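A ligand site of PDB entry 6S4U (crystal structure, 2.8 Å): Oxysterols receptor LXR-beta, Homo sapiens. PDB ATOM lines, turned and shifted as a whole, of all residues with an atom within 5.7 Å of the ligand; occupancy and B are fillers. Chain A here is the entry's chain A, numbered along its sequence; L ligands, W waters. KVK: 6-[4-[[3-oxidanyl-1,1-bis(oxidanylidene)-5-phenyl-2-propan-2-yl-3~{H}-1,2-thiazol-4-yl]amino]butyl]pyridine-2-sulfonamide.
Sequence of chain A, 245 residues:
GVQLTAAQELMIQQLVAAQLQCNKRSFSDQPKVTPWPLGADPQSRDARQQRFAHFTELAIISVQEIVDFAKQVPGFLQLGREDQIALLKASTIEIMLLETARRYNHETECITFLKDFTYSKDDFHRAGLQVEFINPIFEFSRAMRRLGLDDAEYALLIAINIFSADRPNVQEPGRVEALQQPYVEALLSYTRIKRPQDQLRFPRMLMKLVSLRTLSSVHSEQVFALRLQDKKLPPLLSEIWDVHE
The guanidinium group of Arg 103 lies within hydrogen-bond range of an oxygen (O32) of the ligand (2.8 Å). The backbone NH (N) of Leu 114 is in hydrogen-bond range of an oxygen (O31) of the ligand, at 2.8 Å. A nitrogen (N28) of the ligand lies close to the side-chain hydroxyl of Ser 62 (3.2 Å). The side-chain carboxylate (OE1) of Glu 65 sits at hydrogen-bond distance from a nitrogen (N30) of the ligand, at 2.9 Å. An oxygen (O10) of the ligand lies within hydrogen-bond range of a ring nitrogen (NE2) of His 219, at 2.8 Å. A nitrogen (N18) of the ligand is in hydrogen-bond range of the backbone carbonyl oxygen (O) of Phe 55 (3.0 Å).
The side-chain carboxylate (OE1) of Glu 99 lies within salt-bridge range of the guanidinium group (NH1) of Arg 103, at 3.1 Å. OG of Ser 26 lies close to OE2 of Glu 65, at 3.2 Å. OG1 of Thr 100 sits at hydrogen-bond distance from O of Met 96 (2.7 Å). N of Leu 129 is in hydrogen-bond range of O of Phe 124, at 3.3 Å. O of Arg 103 lies within hydrogen-bond range of N of Thr 112 (3.0 Å). The backbone carbonyl oxygen (O) of Phe 52 sits at hydrogen-bond distance from the side-chain hydroxyl (OG1) of Thr 56, 3.0 Å away. The guanidinium group (NH2) of Arg 103 lies within hydrogen-bond range of the side-chain amide oxygen (OD1) of Asn 23 (3.3 Å).
Residues that only touch the ligand: Asn 23 (3.9 Å), Phe 52 (3.9 Å), Thr 56 (3.6 Å), Leu 58 (3.6 Å), Ala 59 (3.6 Å), Ile 93 (3.7 Å), Met 96 (3.5 Å), Glu 99 (3.7 Å), Thr 100 (3.3 Å), Phe 113 (3.5 Å), Phe 124 (3.7 Å), Leu 129 (3.4 Å), Phe 133 (3.2 Å), Leu 226 (3.7 Å), Leu 233 (3.6 Å) and Trp 241 (3.7 Å). Hydrophobic or aromatic side chains that line the ligand: Phe 52, Phe 55, Ala 59, Ile 93, Met 96, Phe 113, Leu 114, Phe 124, Leu 129, Phe 133, His 219, Leu 226, Leu 233 and Trp 241. Within 4 Å of the ligand: Asn 23, Phe 52, Phe 55, Thr 56, Leu 58, Ala 59, Ser 62, Glu 65, Ile 93, Met 96, Glu 99, Thr 100, Arg 103, Phe 113, Leu 114, Phe 124, Leu 129, Phe 133, His 219, Leu 226, Leu 233 and Trp 241. Along chain A the residues within 4 Å of the ligand span positions 23 to 241. The nearest printed residue that does not touch the ligand is Leu 97 (4.04 Å).
Water W2 lies within hydrogen-bond range of the side-chain hydroxyl of Ser 62 (3.2 Å) and an oxygen (O32) of the ligand (3.4 Å).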
ATOM      1  N   ASN A  23     -22.220  38.653   7.427  1.00  0.00           N
ATOM      2  CA  ASN A  23     -22.901  37.888   6.386  1.00  0.00           C
ATOM      3  C   ASN A  23     -22.236  38.069   5.013  1.00  0.00           C
ATOM      4  O   ASN A  23     -22.018  37.083   4.319  1.00  0.00           O
ATOM      5  CB  ASN A  23     -24.390  38.307   6.324  1.00  0.00           C
ATOM      6  CG  ASN A  23     -25.355  37.183   6.007  1.00  0.00           C
ATOM      7  OD1 ASN A  23     -25.362  36.133   6.643  1.00  0.00           O
ATOM      8  ND2 ASN A  23     -26.217  37.407   5.023  1.00  0.00           N
ATOM      9  N   SER A  26     -18.623  36.515   4.759  1.00  0.00           N
ATOM     10  CA  SER A  26     -18.674  35.053   4.907  1.00  0.00           C
ATOM     11  C   SER A  26     -19.037  34.347   3.610  1.00  0.00           C
ATOM     12  O   SER A  26     -18.352  33.402   3.237  1.00  0.00           O
ATOM     13  CB  SER A  26     -19.627  34.657   6.029  1.00  0.00           C
ATOM     14  OG  SER A  26     -19.087  35.159   7.236  1.00  0.00           O
ATOM     15  N   PHE A  52     -19.184  15.245   6.633  1.00  0.00           N
ATOM     16  CA  PHE A  52     -19.010  15.663   8.020  1.00  0.00           C
ATOM     17  C   PHE A  52     -17.970  16.785   8.120  1.00  0.00           C
ATOM     18  O   PHE A  52     -18.169  17.713   8.909  1.00  0.00           O
ATOM     19  CB  PHE A  52     -18.612  14.463   8.897  1.00  0.00           C
ATOM     20  CG  PHE A  52     -18.431  14.773  10.362  1.00  0.00           C
ATOM     21  CD1 PHE A  52     -19.529  14.858  11.215  1.00  0.00           C
ATOM     22  CD2 PHE A  52     -17.164  14.966  10.904  1.00  0.00           C
ATOM     23  CE1 PHE A  52     -19.369  15.133  12.573  1.00  0.00           C
ATOM     24  CE2 PHE A  52     -16.999  15.245  12.255  1.00  0.00           C
ATOM     25  CZ  PHE A  52     -18.102  15.323  13.085  1.00  0.00           C
ATOM     26  N   PHE A  55     -19.635  20.019   6.917  1.00  0.00           N
ATOM     27  CA  PHE A  55     -20.542  20.494   7.946  1.00  0.00           C
ATOM     28  C   PHE A  55     -19.844  21.130   9.140  1.00  0.00           C
ATOM     29  O   PHE A  55     -20.312  22.158   9.640  1.00  0.00           O
ATOM     30  CB  PHE A  55     -21.479  19.361   8.399  1.00  0.00           C
ATOM     31  CG  PHE A  55     -22.942  19.750   8.428  1.00  0.00           C
ATOM     32  CD1 PHE A  55     -23.616  20.089   7.258  1.00  0.00           C
ATOM     33  CD2 PHE A  55     -23.660  19.724   9.616  1.00  0.00           C
ATOM     34  CE1 PHE A  55     -24.969  20.435   7.284  1.00  0.00           C
ATOM     35  CE2 PHE A  55     -25.013  20.070   9.642  1.00  0.00           C
ATOM     36  CZ  PHE A  55     -25.655  20.426   8.476  1.00  0.00           C
ATOM     37  N   THR A  56     -18.708  20.552   9.586  1.00  0.00           N
ATOM     38  CA  THR A  56     -17.914  21.077  10.704  1.00  0.00           C
ATOM     39  C   THR A  56     -17.217  22.380  10.335  1.00  0.00           C
ATOM     40  O   THR A  56     -17.061  23.241  11.186  1.00  0.00           O
ATOM     41  CB  THR A  56     -16.934  20.035  11.244  1.00  0.00           C
ATOM     42  OG1 THR A  56     -16.178  19.501  10.161  1.00  0.00           O
ATOM     43  CG2 THR A  56     -17.619  18.915  12.014  1.00  0.00           C
ATOM     44  N   LEU A  58     -18.419  24.662   8.228  1.00  0.00           N
ATOM     45  CA  LEU A  58     -19.486  25.674   8.219  1.00  0.00           C
ATOM     46  C   LEU A  58     -19.679  26.231   9.628  1.00  0.00           C
ATOM     47  O   LEU A  58     -19.915  27.430   9.788  1.00  0.00           O
ATOM     48  CB  LEU A  58     -20.813  25.095   7.709  1.00  0.00           C
ATOM     49  CG  LEU A  58     -20.887  24.614   6.256  1.00  0.00           C
ATOM     50  CD1 LEU A  58     -22.087  23.737   6.052  1.00  0.00           C
ATOM     51  CD2 LEU A  58     -20.948  25.768   5.280  1.00  0.00           C
ATOM     52  N   ALA A  59     -19.572  25.345  10.646  1.00  0.00           N
ATOM     53  CA  ALA A  59     -19.689  25.686  12.072  1.00  0.00           C
ATOM     54  C   ALA A  59     -18.525  26.598  12.499  1.00  0.00           C
ATOM     55  O   ALA A  59     -18.752  27.574  13.208  1.00  0.00           O
ATOM     56  CB  ALA A  59     -19.711  24.421  12.916  1.00  0.00           C
ATOM     57  N   ILE A  61     -16.833  28.653  10.543  1.00  0.00           N
ATOM     58  CA  ILE A  61     -17.106  29.955   9.927  1.00  0.00           C
ATOM     59  C   ILE A  61     -18.071  30.749  10.818  1.00  0.00           C
ATOM     60  O   ILE A  61     -17.834  31.924  11.076  1.00  0.00           O
ATOM     61  CB  ILE A  61     -17.605  29.823   8.460  1.00  0.00           C
ATOM     62  CG1 ILE A  61     -16.520  29.187   7.564  1.00  0.00           C
ATOM     63  CG2 ILE A  61     -18.081  31.176   7.878  1.00  0.00           C
ATOM     64  CD1 ILE A  61     -17.042  28.427   6.363  1.00  0.00           C
ATOM     65  N   SER A  62     -19.126  30.070  11.329  1.00  0.00           N
ATOM     66  CA  SER A  62     -20.118  30.664  12.226  1.00  0.00           C
ATOM     67  C   SER A  62     -19.516  31.124  13.550  1.00  0.00           C
ATOM     68  O   SER A  62     -19.861  32.216  14.007  1.00  0.00           O
ATOM     69  CB  SER A  62     -21.278  29.716  12.464  1.00  0.00           C
ATOM     70  OG  SER A  62     -22.457  30.251  11.893  1.00  0.00           O
ATOM     71  N   GLU A  65     -17.616  34.234  12.811  1.00  0.00           N
ATOM     72  CA  GLU A  65     -18.627  35.269  12.550  1.00  0.00           C
ATOM     73  C   GLU A  65     -19.189  35.841  13.851  1.00  0.00           C
ATOM     74  O   GLU A  65     -19.302  37.053  13.972  1.00  0.00           O
ATOM     75  CB  GLU A  65     -19.788  34.691  11.729  1.00  0.00           C
ATOM     76  CG  GLU A  65     -19.575  34.722  10.231  1.00  0.00           C
ATOM     77  CD  GLU A  65     -20.773  34.185   9.472  1.00  0.00           C
ATOM     78  OE1 GLU A  65     -20.799  32.961   9.186  1.00  0.00           O
ATOM     79  OE2 GLU A  65     -21.683  34.983   9.159  1.00  0.00           O
ATOM     80  N   ILE A  93     -23.817  28.391  20.164  1.00  0.00           N
ATOM     81  CA  ILE A  93     -24.806  27.474  19.595  1.00  0.00           C
ATOM     82  C   ILE A  93     -26.216  28.094  19.574  1.00  0.00           C
ATOM     83  O   ILE A  93     -26.923  27.930  18.575  1.00  0.00           O
ATOM     84  CB  ILE A  93     -24.788  26.048  20.239  1.00  0.00           C
ATOM     85  CG1 ILE A  93     -25.620  25.032  19.421  1.00  0.00           C
ATOM     86  CG2 ILE A  93     -25.182  26.037  21.723  1.00  0.00           C
ATOM     87  CD1 ILE A  93     -25.194  24.830  17.942  1.00  0.00           C
ATOM     88  N   ILE A  95     -26.906  31.307  19.308  1.00  0.00           N
ATOM     89  CA  ILE A  95     -26.864  32.293  18.220  1.00  0.00           C
ATOM     90  C   ILE A  95     -26.919  31.553  16.884  1.00  0.00           C
ATOM     91  O   ILE A  95     -27.673  31.966  15.993  1.00  0.00           O
ATOM     92  CB  ILE A  95     -25.657  33.268  18.332  1.00  0.00           C
ATOM     93  CG1 ILE A  95     -25.691  34.056  19.661  1.00  0.00           C
ATOM     94  CG2 ILE A  95     -25.609  34.244  17.145  1.00  0.00           C
ATOM     95  CD1 ILE A  95     -24.356  34.573  20.119  1.00  0.00           C
ATOM     96  N   MET A  96     -26.157  30.449  16.748  1.00  0.00           N
ATOM     97  CA  MET A  96     -26.124  29.615  15.550  1.00  0.00           C
ATOM     98  C   MET A  96     -27.533  29.160  15.174  1.00  0.00           C
ATOM     99  O   MET A  96     -27.941  29.343  14.030  1.00  0.00           O
ATOM    100  CB  MET A  96     -25.223  28.383  15.739  1.00  0.00           C
ATOM    101  CG  MET A  96     -23.770  28.642  15.396  1.00  0.00           C
ATOM    102  SD  MET A  96     -22.729  27.243  15.815  1.00  0.00           S
ATOM    103  CE  MET A  96     -22.723  26.394  14.301  1.00  0.00           C
ATOM    104  N   LEU A  97     -28.278  28.639  16.170  1.00  0.00           N
ATOM    105  CA  LEU A  97     -29.649  28.153  16.016  1.00  0.00           C
ATOM    106  C   LEU A  97     -30.627  29.265  15.624  1.00  0.00           C
ATOM    107  O   LEU A  97     -31.501  29.017  14.792  1.00  0.00           O
ATOM    108  CB  LEU A  97     -30.124  27.420  17.277  1.00  0.00           C
ATOM    109  CG  LEU A  97     -29.451  26.084  17.554  1.00  0.00           C
ATOM    110  CD1 LEU A  97     -29.625  25.685  18.992  1.00  0.00           C
ATOM    111  CD2 LEU A  97     -29.939  24.996  16.621  1.00  0.00           C
ATOM    112  N   GLU A  99     -29.813  32.008  13.932  1.00  0.00           N
ATOM    113  CA  GLU A  99     -29.423  32.297  12.548  1.00  0.00           C
ATOM    114  C   GLU A  99     -29.886  31.204  11.601  1.00  0.00           C
ATOM    115  O   GLU A  99     -30.271  31.515  10.480  1.00  0.00           O
ATOM    116  CB  GLU A  99     -27.911  32.546  12.441  1.00  0.00           C
ATOM    117  CG  GLU A  99     -27.437  33.825  13.114  1.00  0.00           C
ATOM    118  CD  GLU A  99     -27.851  35.102  12.405  1.00  0.00           C
ATOM    119  OE1 GLU A  99     -27.099  35.556  11.504  1.00  0.00           O
ATOM    120  OE2 GLU A  99     -28.926  35.647  12.747  1.00  0.00           O
ATOM    121  N   THR A 100     -29.871  29.935  12.066  1.00  0.00           N
ATOM    122  CA  THR A 100     -30.345  28.766  11.321  1.00  0.00           C
ATOM    123  C   THR A 100     -31.855  28.934  11.037  1.00  0.00           C
ATOM    124  O   THR A 100     -32.286  28.776   9.897  1.00  0.00           O
ATOM    125  CB  THR A 100     -30.008  27.475  12.080  1.00  0.00           C
ATOM    126  OG1 THR A 100     -28.600  27.391  12.264  1.00  0.00           O
ATOM    127  CG2 THR A 100     -30.489  26.228  11.371  1.00  0.00           C
ATOM    128  N   ARG A 103     -32.648  31.344   8.284  1.00  0.00           N
ATOM    129  CA  ARG A 103     -32.436  30.895   6.909  1.00  0.00           C
ATOM    130  C   ARG A 103     -33.230  29.626   6.567  1.00  0.00           C
ATOM    131  O   ARG A 103     -32.884  28.911   5.623  1.00  0.00           O
ATOM    132  CB  ARG A 103     -30.937  30.789   6.512  1.00  0.00           C
ATOM    133  CG  ARG A 103     -29.960  30.264   7.545  1.00  0.00           C
ATOM    134  CD  ARG A 103     -28.651  31.055   7.521  1.00  0.00           C
ATOM    135  NE  ARG A 103     -28.754  32.321   8.266  1.00  0.00           N
ATOM    136  CZ  ARG A 103     -27.939  33.353   8.107  1.00  0.00           C
ATOM    137  NH1 ARG A 103     -28.113  34.449   8.839  1.00  0.00           N
ATOM    138  NH2 ARG A 103     -26.943  33.310   7.235  1.00  0.00           N
ATOM    139  N   THR A 112     -30.686  27.319   4.309  1.00  0.00           N
ATOM    140  CA  THR A 112     -29.621  27.739   3.412  1.00  0.00           C
ATOM    141  C   THR A 112     -28.452  28.414   4.141  1.00  0.00           C
ATOM    142  O   THR A 112     -28.543  29.585   4.522  1.00  0.00           O
ATOM    143  CB  THR A 112     -30.167  28.604   2.271  1.00  0.00           C
ATOM    144  OG1 THR A 112     -31.349  27.989   1.728  1.00  0.00           O
ATOM    145  CG2 THR A 112     -29.135  28.821   1.167  1.00  0.00           C
ATOM    146  N   PHE A 113     -27.342  27.678   4.305  1.00  0.00           N
ATOM    147  CA  PHE A 113     -26.120  28.210   4.909  1.00  0.00           C
ATOM    148  C   PHE A 113     -25.290  28.906   3.829  1.00  0.00           C
ATOM    149  O   PHE A 113     -25.243  28.420   2.697  1.00  0.00           O
ATOM    150  CB  PHE A 113     -25.322  27.109   5.624  1.00  0.00           C
ATOM    151  CG  PHE A 113     -26.043  26.419   6.764  1.00  0.00           C
ATOM    152  CD1 PHE A 113     -26.156  25.031   6.801  1.00  0.00           C
ATOM    153  CD2 PHE A 113     -26.608  27.153   7.805  1.00  0.00           C
ATOM    154  CE1 PHE A 113     -26.826  24.393   7.845  1.00  0.00           C
ATOM    155  CE2 PHE A 113     -27.265  26.509   8.852  1.00  0.00           C
ATOM    156  CZ  PHE A 113     -27.378  25.142   8.864  1.00  0.00           C
ATOM    157  N   LEU A 114     -24.703  30.065   4.170  1.00  0.00           N
ATOM    158  CA  LEU A 114     -23.887  30.920   3.305  1.00  0.00           C
ATOM    159  C   LEU A 114     -24.715  31.466   2.119  1.00  0.00           C
ATOM    160  O   LEU A 114     -25.741  32.108   2.367  1.00  0.00           O
ATOM    161  CB  LEU A 114     -22.567  30.233   2.849  1.00  0.00           C
ATOM    162  CG  LEU A 114     -21.608  29.759   3.949  1.00  0.00           C
ATOM    163  CD1 LEU A 114     -20.524  28.895   3.357  1.00  0.00           C
ATOM    164  CD2 LEU A 114     -20.974  30.925   4.696  1.00  0.00           C
ATOM    165  N   PHE A 124     -29.175  16.832   6.592  1.00  0.00           N
ATOM    166  CA  PHE A 124     -28.636  16.953   7.951  1.00  0.00           C
ATOM    167  C   PHE A 124     -28.268  15.581   8.509  1.00  0.00           C
ATOM    168  O   PHE A 124     -27.257  15.457   9.215  1.00  0.00           O
ATOM    169  CB  PHE A 124     -29.665  17.636   8.876  1.00  0.00           C
ATOM    170  CG  PHE A 124     -29.611  19.143   8.885  1.00  0.00           C
ATOM    171  CD1 PHE A 124     -30.292  19.887   7.932  1.00  0.00           C
ATOM    172  CD2 PHE A 124     -28.916  19.824   9.874  1.00  0.00           C
ATOM    173  CE1 PHE A 124     -30.245  21.282   7.940  1.00  0.00           C
ATOM    174  CE2 PHE A 124     -28.874  21.227   9.885  1.00  0.00           C
ATOM    175  CZ  PHE A 124     -29.543  21.936   8.914  1.00  0.00           C
ATOM    176  N   LEU A 129     -25.921  13.726  11.702  1.00  0.00           N
ATOM    177  CA  LEU A 129     -26.654  14.206  12.872  1.00  0.00           C
ATOM    178  C   LEU A 129     -27.822  13.303  13.248  1.00  0.00           C
ATOM    179  O   LEU A 129     -28.424  12.674  12.368  1.00  0.00           O
ATOM    180  CB  LEU A 129     -27.129  15.652  12.688  1.00  0.00           C
ATOM    181  CG  LEU A 129     -26.069  16.746  12.518  1.00  0.00           C
ATOM    182  CD1 LEU A 129     -26.715  18.073  12.212  1.00  0.00           C
ATOM    183  CD2 LEU A 129     -25.200  16.897  13.760  1.00  0.00           C
ATOM    184  N   PHE A 133     -31.852  15.573  17.410  1.00  0.00           N
ATOM    185  CA  PHE A 133     -31.359  16.945  17.293  1.00  0.00           C
ATOM    186  C   PHE A 133     -31.869  17.654  16.035  1.00  0.00           C
ATOM    187  O   PHE A 133     -32.061  18.860  16.076  1.00  0.00           O
ATOM    188  CB  PHE A 133     -29.817  17.000  17.411  1.00  0.00           C
ATOM    189  CG  PHE A 133     -29.183  18.376  17.315  1.00  0.00           C
ATOM    190  CD1 PHE A 133     -29.543  19.386  18.187  1.00  0.00           C
ATOM    191  CD2 PHE A 133     -28.182  18.625  16.380  1.00  0.00           C
ATOM    192  CE1 PHE A 133     -28.941  20.654  18.104  1.00  0.00           C
ATOM    193  CE2 PHE A 133     -27.585  19.887  16.305  1.00  0.00           C
ATOM    194  CZ  PHE A 133     -27.967  20.891  17.158  1.00  0.00           C
ATOM    195  N   ILE A 137     -34.425  21.333  15.630  1.00  0.00           N
ATOM    196  CA  ILE A 137     -33.903  22.423  14.777  1.00  0.00           C
ATOM    197  C   ILE A 137     -35.014  22.966  13.882  1.00  0.00           C
ATOM    198  O   ILE A 137     -35.295  24.156  13.924  1.00  0.00           O
ATOM    199  CB  ILE A 137     -32.622  22.006  13.967  1.00  0.00           C
ATOM    200  CG1 ILE A 137     -31.352  21.834  14.828  1.00  0.00           C
ATOM    201  CG2 ILE A 137     -32.323  22.984  12.814  1.00  0.00           C
ATOM    202  CD1 ILE A 137     -31.464  21.875  16.291  1.00  0.00           C
ATOM    203  N   HIS A 219     -27.989  19.778  21.834  1.00  0.00           N
ATOM    204  CA  HIS A 219     -26.747  19.903  21.071  1.00  0.00           C
ATOM    205  C   HIS A 219     -25.572  19.263  21.827  1.00  0.00           C
ATOM    206  O   HIS A 219     -24.711  18.661  21.187  1.00  0.00           O
ATOM    207  CB  HIS A 219     -26.450  21.376  20.753  1.00  0.00           C
ATOM    208  CG  HIS A 219     -25.134  21.593  20.060  1.00  0.00           C
ATOM    209  ND1 HIS A 219     -24.027  22.026  20.756  1.00  0.00           N
ATOM    210  CD2 HIS A 219     -24.790  21.375  18.766  1.00  0.00           C
ATOM    211  CE1 HIS A 219     -23.053  22.097  19.869  1.00  0.00           C
ATOM    212  NE2 HIS A 219     -23.464  21.708  18.660  1.00  0.00           N
ATOM    213  N   GLN A 222     -25.850  15.630  21.355  1.00  0.00           N
ATOM    214  CA  GLN A 222     -25.438  15.344  19.987  1.00  0.00           C
ATOM    215  C   GLN A 222     -23.914  15.188  19.914  1.00  0.00           C
ATOM    216  O   GLN A 222     -23.431  14.262  19.249  1.00  0.00           O
ATOM    217  CB  GLN A 222     -25.937  16.454  19.023  1.00  0.00           C
ATOM    218  CG  GLN A 222     -25.411  16.380  17.588  1.00  0.00           C
ATOM    219  CD  GLN A 222     -25.877  15.157  16.836  1.00  0.00           C
ATOM    220  OE1 GLN A 222     -27.004  15.106  16.331  1.00  0.00           O
ATOM    221  NE2 GLN A 222     -25.018  14.158  16.738  1.00  0.00           N
ATOM    222  N   VAL A 223     -23.165  16.078  20.605  1.00  0.00           N
ATOM    223  CA  VAL A 223     -21.694  16.052  20.661  1.00  0.00           C
ATOM    224  C   VAL A 223     -21.211  14.803  21.406  1.00  0.00           C
ATOM    225  O   VAL A 223     -20.285  14.131  20.936  1.00  0.00           O
ATOM    226  CB  VAL A 223     -21.115  17.378  21.241  1.00  0.00           C
ATOM    227  CG1 VAL A 223     -19.604  17.278  21.435  1.00  0.00           C
ATOM    228  CG2 VAL A 223     -21.457  18.566  20.348  1.00  0.00           C
ATOM    229  N   LEU A 226     -21.411  11.772  19.235  1.00  0.00           N
ATOM    230  CA  LEU A 226     -20.339  11.735  18.235  1.00  0.00           C
ATOM    231  C   LEU A 226     -19.065  11.082  18.782  1.00  0.00           C
ATOM    232  O   LEU A 226     -18.334  10.444  18.022  1.00  0.00           O
ATOM    233  CB  LEU A 226     -20.014  13.129  17.671  1.00  0.00           C
ATOM    234  CG  LEU A 226     -21.081  13.796  16.809  1.00  0.00           C
ATOM    235  CD1 LEU A 226     -20.830  15.278  16.702  1.00  0.00           C
ATOM    236  CD2 LEU A 226     -21.132  13.177  15.410  1.00  0.00           C
ATOM    237  N   LEU A 233     -14.198  16.091  16.632  1.00  0.00           N
ATOM    238  CA  LEU A 233     -14.453  17.479  16.253  1.00  0.00           C
ATOM    239  C   LEU A 233     -13.144  18.219  15.959  1.00  0.00           C
ATOM    240  O   LEU A 233     -12.144  17.962  16.645  1.00  0.00           O
ATOM    241  CB  LEU A 233     -15.208  18.232  17.370  1.00  0.00           C
ATOM    242  CG  LEU A 233     -16.593  17.713  17.804  1.00  0.00           C
ATOM    243  CD1 LEU A 233     -17.167  18.612  18.876  1.00  0.00           C
ATOM    244  CD2 LEU A 233     -17.548  17.631  16.640  1.00  0.00           C
ATOM    245  N   LEU A 237     -13.790  23.752  17.312  1.00  0.00           N
ATOM    246  CA  LEU A 237     -15.092  23.330  17.853  1.00  0.00           C
ATOM    247  C   LEU A 237     -14.981  22.513  19.129  1.00  0.00           C
ATOM    248  O   LEU A 237     -15.886  22.551  19.958  1.00  0.00           O
ATOM    249  CB  LEU A 237     -15.920  22.571  16.793  1.00  0.00           C
ATOM    250  CG  LEU A 237     -16.147  23.253  15.431  1.00  0.00           C
ATOM    251  CD1 LEU A 237     -16.852  22.323  14.477  1.00  0.00           C
ATOM    252  CD2 LEU A 237     -16.924  24.555  15.563  1.00  0.00           C
ATOM    253  N   TRP A 241     -17.177  23.052  22.559  1.00  0.00           N
ATOM    254  CA  TRP A 241     -18.183  22.017  22.819  1.00  0.00           C
ATOM    255  C   TRP A 241     -17.656  20.668  23.339  1.00  0.00           C
ATOM    256  O   TRP A 241     -18.057  19.629  22.827  1.00  0.00           O
ATOM    257  CB  TRP A 241     -19.042  21.795  21.559  1.00  0.00           C
ATOM    258  CG  TRP A 241     -19.672  23.033  20.977  1.00  0.00           C
ATOM    259  CD1 TRP A 241     -20.214  24.084  21.668  1.00  0.00           C
ATOM    260  CD2 TRP A 241     -19.907  23.306  19.593  1.00  0.00           C
ATOM    261  NE1 TRP A 241     -20.720  25.014  20.792  1.00  0.00           N
ATOM    262  CE2 TRP A 241     -20.564  24.548  19.507  1.00  0.00           C
ATOM    263  CE3 TRP A 241     -19.628  22.613  18.402  1.00  0.00           C
ATOM    264  CZ2 TRP A 241     -20.935  25.132  18.288  1.00  0.00           C
ATOM    265  CZ3 TRP A 241     -19.999  23.183  17.187  1.00  0.00           C
ATOM    266  CH2 TRP A 241     -20.636  24.424  17.141  1.00  0.00           C
HETATM  267  C1  KVK L   1     -23.030  21.870  12.580  1.00  0.00           C
HETATM  268  C2  KVK L   1     -24.072  22.108  13.438  1.00  0.00           C
HETATM  269  C7  KVK L   1     -21.565  19.321  15.059  1.00  0.00           C
HETATM  270  C8  KVK L   1     -21.416  18.005  14.292  1.00  0.00           C
HETATM  271  C9  KVK L   1     -20.222  19.856  15.548  1.00  0.00           C
HETATM  272  C12 KVK L   1     -25.272  22.950  13.376  1.00  0.00           C
HETATM  273  C13 KVK L   1     -25.439  24.006  14.305  1.00  0.00           C
HETATM  274  C14 KVK L   1     -26.598  24.774  14.284  1.00  0.00           C
HETATM  275  C15 KVK L   1     -27.606  24.488  13.368  1.00  0.00           C
HETATM  276  C16 KVK L   1     -27.467  23.428  12.475  1.00  0.00           C
HETATM  277  N18 KVK L   1     -22.808  22.389  11.297  1.00  0.00           N
HETATM  278  C19 KVK L   1     -23.583  23.398  10.572  1.00  0.00           C
HETATM  279  C20 KVK L   1     -23.107  24.757  11.055  1.00  0.00           C
HETATM  280  C21 KVK L   1     -24.170  25.806  10.772  1.00  0.00           C
HETATM  281  C22 KVK L   1     -23.444  27.003  10.165  1.00  0.00           C
HETATM  282  C24 KVK L   1     -25.237  28.491  11.175  1.00  0.00           C
HETATM  283  C27 KVK L   1     -24.690  30.337   9.240  1.00  0.00           C
HETATM  284  S3  KVK L   1     -23.672  21.082  14.828  1.00  0.00           S
HETATM  285  N4  KVK L   1     -22.294  20.328  14.278  1.00  0.00           N
HETATM  286  C5  KVK L   1     -22.065  20.886  13.069  1.00  0.00           C
HETATM  287  O6  KVK L   1     -21.123  20.561  12.361  1.00  0.00           O
HETATM  288  O10 KVK L   1     -23.285  21.934  15.886  1.00  0.00           O
HETATM  289  O11 KVK L   1     -24.672  20.071  14.928  1.00  0.00           O
HETATM  290  C17 KVK L   1     -26.327  22.637  12.495  1.00  0.00           C
HETATM  291  C23 KVK L   1     -24.270  28.263  10.195  1.00  0.00           C
HETATM  292  C25 KVK L   1     -25.964  29.680  11.160  1.00  0.00           C
HETATM  293  C26 KVK L   1     -25.676  30.630  10.173  1.00  0.00           C
HETATM  294  N28 KVK L   1     -24.020  29.191   9.278  1.00  0.00           N
HETATM  295  S29 KVK L   1     -24.280  31.501   7.985  1.00  0.00           S
HETATM  296  N30 KVK L   1     -22.651  31.325   7.729  1.00  0.00           N
HETATM  297  O31 KVK L   1     -24.920  31.041   6.802  1.00  0.00           O
HETATM  298  O32 KVK L   1     -24.493  32.797   8.532  1.00  0.00           O
HETATM  299  O   HOH W   1     -24.332  35.791   9.356  1.00  0.00           O
HETATM  300  O   HOH W   2     -23.685  33.217  11.846  1.00  0.00           O
